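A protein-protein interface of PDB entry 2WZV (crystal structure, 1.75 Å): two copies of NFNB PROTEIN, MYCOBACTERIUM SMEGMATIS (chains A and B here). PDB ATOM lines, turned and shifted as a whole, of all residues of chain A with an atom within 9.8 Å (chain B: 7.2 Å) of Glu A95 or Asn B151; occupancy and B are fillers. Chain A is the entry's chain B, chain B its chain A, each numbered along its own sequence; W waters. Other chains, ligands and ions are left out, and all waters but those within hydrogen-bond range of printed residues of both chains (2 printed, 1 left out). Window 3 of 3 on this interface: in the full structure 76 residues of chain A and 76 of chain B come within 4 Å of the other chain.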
ATOM      1  N   PRO A  92      -2.934 -35.365  25.560  1.00  0.00           N
ATOM      2  CA  PRO A  92      -2.366 -35.678  26.900  1.00  0.00           C
ATOM      3  C   PRO A  92      -2.009 -34.427  27.703  1.00  0.00           C
ATOM      4  O   PRO A  92      -1.828 -33.344  27.118  1.00  0.00           O
ATOM      5  CB  PRO A  92      -1.123 -36.499  26.581  1.00  0.00           C
ATOM      6  CG  PRO A  92      -0.726 -36.096  25.193  1.00  0.00           C
ATOM      7  CD  PRO A  92      -2.000 -35.720  24.473  1.00  0.00           C
ATOM      8  N   TYR A  93      -1.899 -34.559  29.023  1.00  0.00           N
ATOM      9  CA  TYR A  93      -1.516 -33.435  29.867  1.00  0.00           C
ATOM     10  C   TYR A  93      -0.005 -33.218  29.718  1.00  0.00           C
ATOM     11  O   TYR A  93       0.720 -34.156  29.392  1.00  0.00           O
ATOM     12  CB  TYR A  93      -1.864 -33.725  31.349  1.00  0.00           C
ATOM     13  CG  TYR A  93      -1.717 -32.530  32.274  1.00  0.00           C
ATOM     14  CD1 TYR A  93      -2.558 -31.423  32.159  1.00  0.00           C
ATOM     15  CD2 TYR A  93      -0.768 -32.523  33.288  1.00  0.00           C
ATOM     16  CE1 TYR A  93      -2.425 -30.321  33.006  1.00  0.00           C
ATOM     17  CE2 TYR A  93      -0.638 -31.432  34.152  1.00  0.00           C
ATOM     18  CZ  TYR A  93      -1.471 -30.335  34.008  1.00  0.00           C
ATOM     19  OH  TYR A  93      -1.353 -29.257  34.852  1.00  0.00           O
ATOM     20  N   ARG A  94       0.457 -31.992  29.926  1.00  0.00           N
ATOM     21  CA  ARG A  94       1.885 -31.713  29.884  1.00  0.00           C
ATOM     22  C   ARG A  94       2.301 -31.198  31.247  1.00  0.00           C
ATOM     23  O   ARG A  94       1.703 -30.261  31.781  1.00  0.00           O
ATOM     24  CB  ARG A  94       2.282 -30.758  28.741  1.00  0.00           C
ATOM     25  CG  ARG A  94       3.797 -30.670  28.554  1.00  0.00           C
ATOM     26  CD  ARG A  94       4.209 -30.219  27.170  1.00  0.00           C
ATOM     27  NE  ARG A  94       5.593 -29.741  27.164  1.00  0.00           N
ATOM     28  CZ  ARG A  94       6.262 -29.385  26.074  1.00  0.00           C
ATOM     29  NH1 ARG A  94       5.688 -29.458  24.879  1.00  0.00           N
ATOM     30  NH2 ARG A  94       7.514 -28.956  26.167  1.00  0.00           N
ATOM     31  N   GLU A  95       3.293 -31.847  31.830  1.00  0.00           N
ATOM     32  CA  GLU A  95       3.795 -31.500  33.148  1.00  0.00           C
ATOM     33  C   GLU A  95       4.200 -30.031  33.264  1.00  0.00           C
ATOM     34  O   GLU A  95       4.782 -29.464  32.329  1.00  0.00           O
ATOM     35  CB  GLU A  95       4.944 -32.412  33.510  1.00  0.00           C
ATOM     36  CG  GLU A  95       5.080 -32.578  34.998  1.00  0.00           C
ATOM     37  CD  GLU A  95       6.266 -33.436  35.347  1.00  0.00           C
ATOM     38  OE1 GLU A  95       6.329 -34.593  34.870  1.00  0.00           O
ATOM     39  OE2 GLU A  95       7.141 -32.941  36.090  1.00  0.00           O
ATOM     40  N   GLY A  96       3.824 -29.431  34.394  1.00  0.00           N
ATOM     41  CA  GLY A  96       4.075 -28.032  34.705  1.00  0.00           C
ATOM     42  C   GLY A  96       3.254 -27.072  33.868  1.00  0.00           C
ATOM     43  O   GLY A  96       3.639 -25.908  33.724  1.00  0.00           O
ATOM     44  N   LEU A  97       2.107 -27.550  33.320  1.00  0.00           N
ATOM     45  CA  LEU A  97       1.205 -26.753  32.482  1.00  0.00           C
ATOM     46  C   LEU A  97       0.881 -25.386  33.103  1.00  0.00           C
ATOM     47  O   LEU A  97       0.966 -24.373  32.408  1.00  0.00           O
ATOM     48  CB  LEU A  97      -0.087 -27.523  32.192  1.00  0.00           C
ATOM     49  N   PHE A  98       0.538 -25.362  34.408  1.00  0.00           N
ATOM     50  CA  PHE A  98       0.198 -24.131  35.119  1.00  0.00           C
ATOM     51  C   PHE A  98       1.144 -23.871  36.291  1.00  0.00           C
ATOM     52  O   PHE A  98       0.946 -24.382  37.397  1.00  0.00           O
ATOM     53  CB  PHE A  98      -1.285 -24.117  35.555  1.00  0.00           C
ATOM     54  CG  PHE A  98      -2.313 -24.390  34.476  1.00  0.00           C
ATOM     55  CD1 PHE A  98      -2.186 -23.827  33.208  1.00  0.00           C
ATOM     56  CD2 PHE A  98      -3.436 -25.158  34.745  1.00  0.00           C
ATOM     57  CE1 PHE A  98      -3.132 -24.088  32.215  1.00  0.00           C
ATOM     58  CE2 PHE A  98      -4.398 -25.391  33.761  1.00  0.00           C
ATOM     59  CZ  PHE A  98      -4.240 -24.857  32.504  1.00  0.00           C
ATOM     60  N   GLN A  99       2.195 -23.093  36.018  1.00  0.00           N
ATOM     61  CA  GLN A  99       3.220 -22.701  36.986  1.00  0.00           C
ATOM     62  C   GLN A  99       3.150 -21.193  37.193  1.00  0.00           C
ATOM     63  O   GLN A  99       2.817 -20.465  36.254  1.00  0.00           O
ATOM     64  CB  GLN A  99       4.617 -23.071  36.465  1.00  0.00           C
ATOM     65  CG  GLN A  99       4.934 -24.564  36.485  1.00  0.00           C
ATOM     66  CD  GLN A  99       6.134 -24.929  35.635  1.00  0.00           C
ATOM     67  OE1 GLN A  99       6.515 -24.225  34.685  1.00  0.00           O
ATOM     68  NE2 GLN A  99       6.744 -26.065  35.940  1.00  0.00           N
ATOM     69  N   GLY A 100       3.472 -20.747  38.411  1.00  0.00           N
ATOM     70  CA  GLY A 100       3.493 -19.338  38.782  1.00  0.00           C
ATOM     71  C   GLY A 100       2.156 -18.645  38.623  1.00  0.00           C
ATOM     72  O   GLY A 100       1.135 -19.124  39.135  1.00  0.00           O
ATOM     73  N   LEU A 102       0.103 -18.497  36.145  1.00  0.00           N
ATOM     74  CA  LEU A 102      -0.958 -19.306  35.506  1.00  0.00           C
ATOM     75  C   LEU A 102      -1.718 -20.099  36.556  1.00  0.00           C
ATOM     76  O   LEU A 102      -2.948 -20.183  36.489  1.00  0.00           O
ATOM     77  CB  LEU A 102      -0.440 -20.250  34.393  1.00  0.00           C
ATOM     78  CG  LEU A 102       0.367 -19.657  33.210  1.00  0.00           C
ATOM     79  CD1 LEU A 102       0.373 -20.628  32.025  1.00  0.00           C
ATOM     80  CD2 LEU A 102      -0.199 -18.328  32.714  1.00  0.00           C
ATOM     81  N   ALA A 154       0.607 -27.771  18.139  1.00  0.00           N
ATOM     82  CA  ALA A 154       0.376 -26.385  18.543  1.00  0.00           C
ATOM     83  C   ALA A 154      -0.144 -25.461  17.458  1.00  0.00           C
ATOM     84  O   ALA A 154      -1.102 -24.727  17.714  1.00  0.00           O
ATOM     85  CB  ALA A 154       1.621 -25.805  19.190  1.00  0.00           C
ATOM     86  N   PHE B  91       8.060 -24.187  17.499  1.00  0.00           N
ATOM     87  CA  PHE B  91       6.961 -25.105  17.202  1.00  0.00           C
ATOM     88  C   PHE B  91       7.175 -25.629  15.779  1.00  0.00           C
ATOM     89  O   PHE B  91       6.980 -24.875  14.834  1.00  0.00           O
ATOM     90  CB  PHE B  91       5.605 -24.389  17.324  1.00  0.00           C
ATOM     91  CG  PHE B  91       5.307 -23.866  18.705  1.00  0.00           C
ATOM     92  CD1 PHE B  91       4.950 -24.733  19.733  1.00  0.00           C
ATOM     93  CD2 PHE B  91       5.407 -22.510  18.988  1.00  0.00           C
ATOM     94  CE1 PHE B  91       4.656 -24.245  21.013  1.00  0.00           C
ATOM     95  CE2 PHE B  91       5.125 -22.023  20.266  1.00  0.00           C
ATOM     96  CZ  PHE B  91       4.754 -22.891  21.270  1.00  0.00           C
ATOM     97  N   ALA B 148       4.260 -17.581  24.020  1.00  0.00           N
ATOM     98  CA  ALA B 148       3.538 -18.584  24.770  1.00  0.00           C
ATOM     99  C   ALA B 148       4.449 -19.252  25.805  1.00  0.00           C
ATOM    100  O   ALA B 148       5.683 -19.162  25.685  1.00  0.00           O
ATOM    101  CB  ALA B 148       2.965 -19.616  23.796  1.00  0.00           C
ATOM    102  N   PRO B 149       3.878 -19.910  26.844  1.00  0.00           N
ATOM    103  CA  PRO B 149       4.730 -20.592  27.831  1.00  0.00           C
ATOM    104  C   PRO B 149       5.667 -21.635  27.200  1.00  0.00           C
ATOM    105  O   PRO B 149       5.388 -22.192  26.130  1.00  0.00           O
ATOM    106  CB  PRO B 149       3.726 -21.293  28.754  1.00  0.00           C
ATOM    107  CG  PRO B 149       2.463 -20.477  28.640  1.00  0.00           C
ATOM    108  CD  PRO B 149       2.437 -20.050  27.182  1.00  0.00           C
ATOM    109  N   ASN B 150       6.794 -21.897  27.874  1.00  0.00           N
ATOM    110  CA  ASN B 150       7.773 -22.884  27.405  1.00  0.00           C
ATOM    111  C   ASN B 150       7.175 -24.265  27.186  1.00  0.00           C
ATOM    112  O   ASN B 150       7.584 -24.969  26.262  1.00  0.00           O
ATOM    113  CB  ASN B 150       8.924 -23.007  28.424  1.00  0.00           C
ATOM    114  CG  ASN B 150      10.189 -22.324  27.996  1.00  0.00           C
ATOM    115  OD1 ASN B 150      10.255 -21.660  26.953  1.00  0.00           O
ATOM    116  ND2 ASN B 150      11.220 -22.451  28.815  1.00  0.00           N
ATOM    117  N   ASN B 151       6.221 -24.665  28.039  1.00  0.00           N
ATOM    118  CA  ASN B 151       5.620 -25.992  27.937  1.00  0.00           C
ATOM    119  C   ASN B 151       4.324 -26.038  27.121  1.00  0.00           C
ATOM    120  O   ASN B 151       3.552 -26.992  27.245  1.00  0.00           O
ATOM    121  CB  ASN B 151       5.461 -26.612  29.332  1.00  0.00           C
ATOM    122  CG  ASN B 151       6.774 -26.832  30.055  1.00  0.00           C
ATOM    123  OD1 ASN B 151       7.758 -27.329  29.492  1.00  0.00           O
ATOM    124  ND2 ASN B 151       6.810 -26.484  31.329  1.00  0.00           N
ATOM    125  N   THR B 152       4.096 -25.025  26.246  1.00  0.00           N
ATOM    126  CA  THR B 152       2.893 -24.972  25.412  1.00  0.00           C
ATOM    127  C   THR B 152       2.656 -26.277  24.653  1.00  0.00           C
ATOM    128  O   THR B 152       3.572 -26.805  24.023  1.00  0.00           O
ATOM    129  CB  THR B 152       2.967 -23.794  24.436  1.00  0.00           C
ATOM    130  OG1 THR B 152       2.930 -22.606  25.208  1.00  0.00           O
ATOM    131  CG2 THR B 152       1.805 -23.790  23.403  1.00  0.00           C
ATOM    132  N   GLU B 153       1.423 -26.765  24.719  1.00  0.00           N
ATOM    133  CA  GLU B 153       0.934 -27.919  23.975  1.00  0.00           C
ATOM    134  C   GLU B 153      -0.369 -27.483  23.277  1.00  0.00           C
ATOM    135  O   GLU B 153      -0.627 -26.280  23.185  1.00  0.00           O
ATOM    136  CB  GLU B 153       0.783 -29.194  24.861  1.00  0.00           C
ATOM    137  CG  GLU B 153       0.184 -29.020  26.245  1.00  0.00           C
ATOM    138  CD  GLU B 153      -1.161 -28.329  26.256  1.00  0.00           C
ATOM    139  OE1 GLU B 153      -2.194 -29.022  26.107  1.00  0.00           O
ATOM    140  OE2 GLU B 153      -1.164 -27.077  26.272  1.00  0.00           O
ATOM    141  N   ALA B 154      -1.188 -28.427  22.790  1.00  0.00           N
ATOM    142  CA  ALA B 154      -2.402 -28.096  22.056  1.00  0.00           C
ATOM    143  C   ALA B 154      -3.395 -27.174  22.774  1.00  0.00           C
ATOM    144  O   ALA B 154      -3.890 -26.234  22.161  1.00  0.00           O
ATOM    145  CB  ALA B 154      -3.099 -29.358  21.570  1.00  0.00           C
ATOM    146  N   ILE B 156      -3.008 -24.978  25.427  1.00  0.00           N
ATOM    147  CA  ILE B 156      -2.461 -23.634  25.600  1.00  0.00           C
ATOM    148  C   ILE B 156      -2.400 -22.945  24.223  1.00  0.00           C
ATOM    149  O   ILE B 156      -2.794 -21.779  24.112  1.00  0.00           O
ATOM    150  CB  ILE B 156      -1.079 -23.649  26.284  1.00  0.00           C
ATOM    151  CG1 ILE B 156      -1.196 -24.066  27.777  1.00  0.00           C
ATOM    152  CG2 ILE B 156      -0.414 -22.272  26.145  1.00  0.00           C
ATOM    153  CD1 ILE B 156       0.184 -24.104  28.544  1.00  0.00           C
ATOM    154  N   ASN B 199      12.793 -17.731  27.967  1.00  0.00           N
ATOM    155  CA  ASN B 199      11.911 -18.743  28.550  1.00  0.00           C
ATOM    156  C   ASN B 199      10.455 -18.619  28.144  1.00  0.00           C
ATOM    157  O   ASN B 199       9.568 -18.864  28.954  1.00  0.00           O
ATOM    158  CB  ASN B 199      12.070 -18.767  30.089  1.00  0.00           C
ATOM    159  CG  ASN B 199      13.493 -19.028  30.514  1.00  0.00           C
ATOM    160  OD1 ASN B 199      14.131 -19.984  30.065  1.00  0.00           O
ATOM    161  ND2 ASN B 199      14.045 -18.144  31.334  1.00  0.00           N
ATOM    162  N   LYS B 201       8.066 -19.293  24.306  1.00  0.00           N
ATOM    163  CA  LYS B 201       8.109 -19.775  22.927  1.00  0.00           C
ATOM    164  C   LYS B 201       7.324 -18.850  22.029  1.00  0.00           C
ATOM    165  O   LYS B 201       6.282 -18.339  22.436  1.00  0.00           O
ATOM    166  CB  LYS B 201       7.584 -21.220  22.854  1.00  0.00           C
ATOM    167  CG  LYS B 201       8.618 -22.203  23.419  1.00  0.00           C
ATOM    168  CD  LYS B 201       8.194 -23.654  23.182  1.00  0.00           C
ATOM    169  CE  LYS B 201       9.321 -24.584  23.597  1.00  0.00           C
ATOM    170  NZ  LYS B 201       8.821 -25.964  23.805  1.00  0.00           N
HETATM  171  O   HOH W   1      -2.080 -31.583  25.280  1.00  0.00           O
HETATM  172  O   HOH W   2       6.132 -26.717  24.110  1.00  0.00           O
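The guanidinium group (NE) of Arg A94 sits close to the backbone carbonyl oxygen (O) of Asn B151 (3.4 Å). O of Thr B152 is in hydrogen-bond range of NH1 of Arg A94.
The backbone carbonyl oxygen (O) of Pro B149 is in hydrogen-bond range of the side-chain hydroxyl (OG1) of Thr B152 (2.7 Å). The backbone carbonyl oxygen of Asn B150 lies within hydrogen-bond range of the side-chain amino group of Lys B201, at 2.9 Å. The side-chain carboxylate (OE2) of Glu B153 lies within hydrogen-bond range of the backbone NH (N) of Ile B156 (2.9 Å).
Among the printed residues, merely in contact across the chains: Ala A154 with Phe B91, Arg A94 with Glu B153, Glu A95 with Asn B151, Leu A97 with Ile B156, Leu A102 with Pro B149 and Arg A94 with Asn B150.
Of the printed residues of chain A, Asn B151 touches Arg A94 (3.3 Å) and Glu A95 (3.7 Å). Printed residues of chain A within 4 Å of Phe B91: Ala A154 (3.5 Å). Printed residues of chain B within 4 Å of Leu A97: Ile B156 (3.95 Å). Printed residues of chain B within 4 Å of Ala A154: Phe B91. Printed residues of chain B within 4 Å of Arg A94: Asn B150, Asn B151, Thr B152 and Glu B153. Printed residues of chain A within 4 Å of Asn B150: Arg A94. The nearest printed residue of chain B that does not touch Ala A154 is Glu B153 (4.6 Å).
Of the 11 printed residues of chain A, 5 touch a printed residue of chain B. Printed residues of chain A that touch a printed residue of chain B: Arg A94, Glu A95, Leu A97, Leu A102 and Ala A154. Hydrophobic or aromatic side chains of chain A within 4 Å of the printed part of chain B: Leu A102 and Ala A154. Among the printed residues, 8 pairs touch across the chains.
Position printed for both chains: 154. Of the 8 pairs that touch across the chains among the printed residues, none has its exchanged pair printed and touching as well.
Water W1 lies within hydrogen-bond range of O of Pro A92 (2.6 Å) and OE1 of Glu B153 (2.7 Å). Water W2 lies within hydrogen-bond range of the backbone carbonyl oxygen (O) of Thr B152 (2.6 Å), the side-chain amino group (NZ) of Lys B201 (2.8 Å), the guanidinium group (NH1) of Arg A94 (2.9 Å) and the backbone carbonyl oxygen (O) of Asn B150 (3.1 Å).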
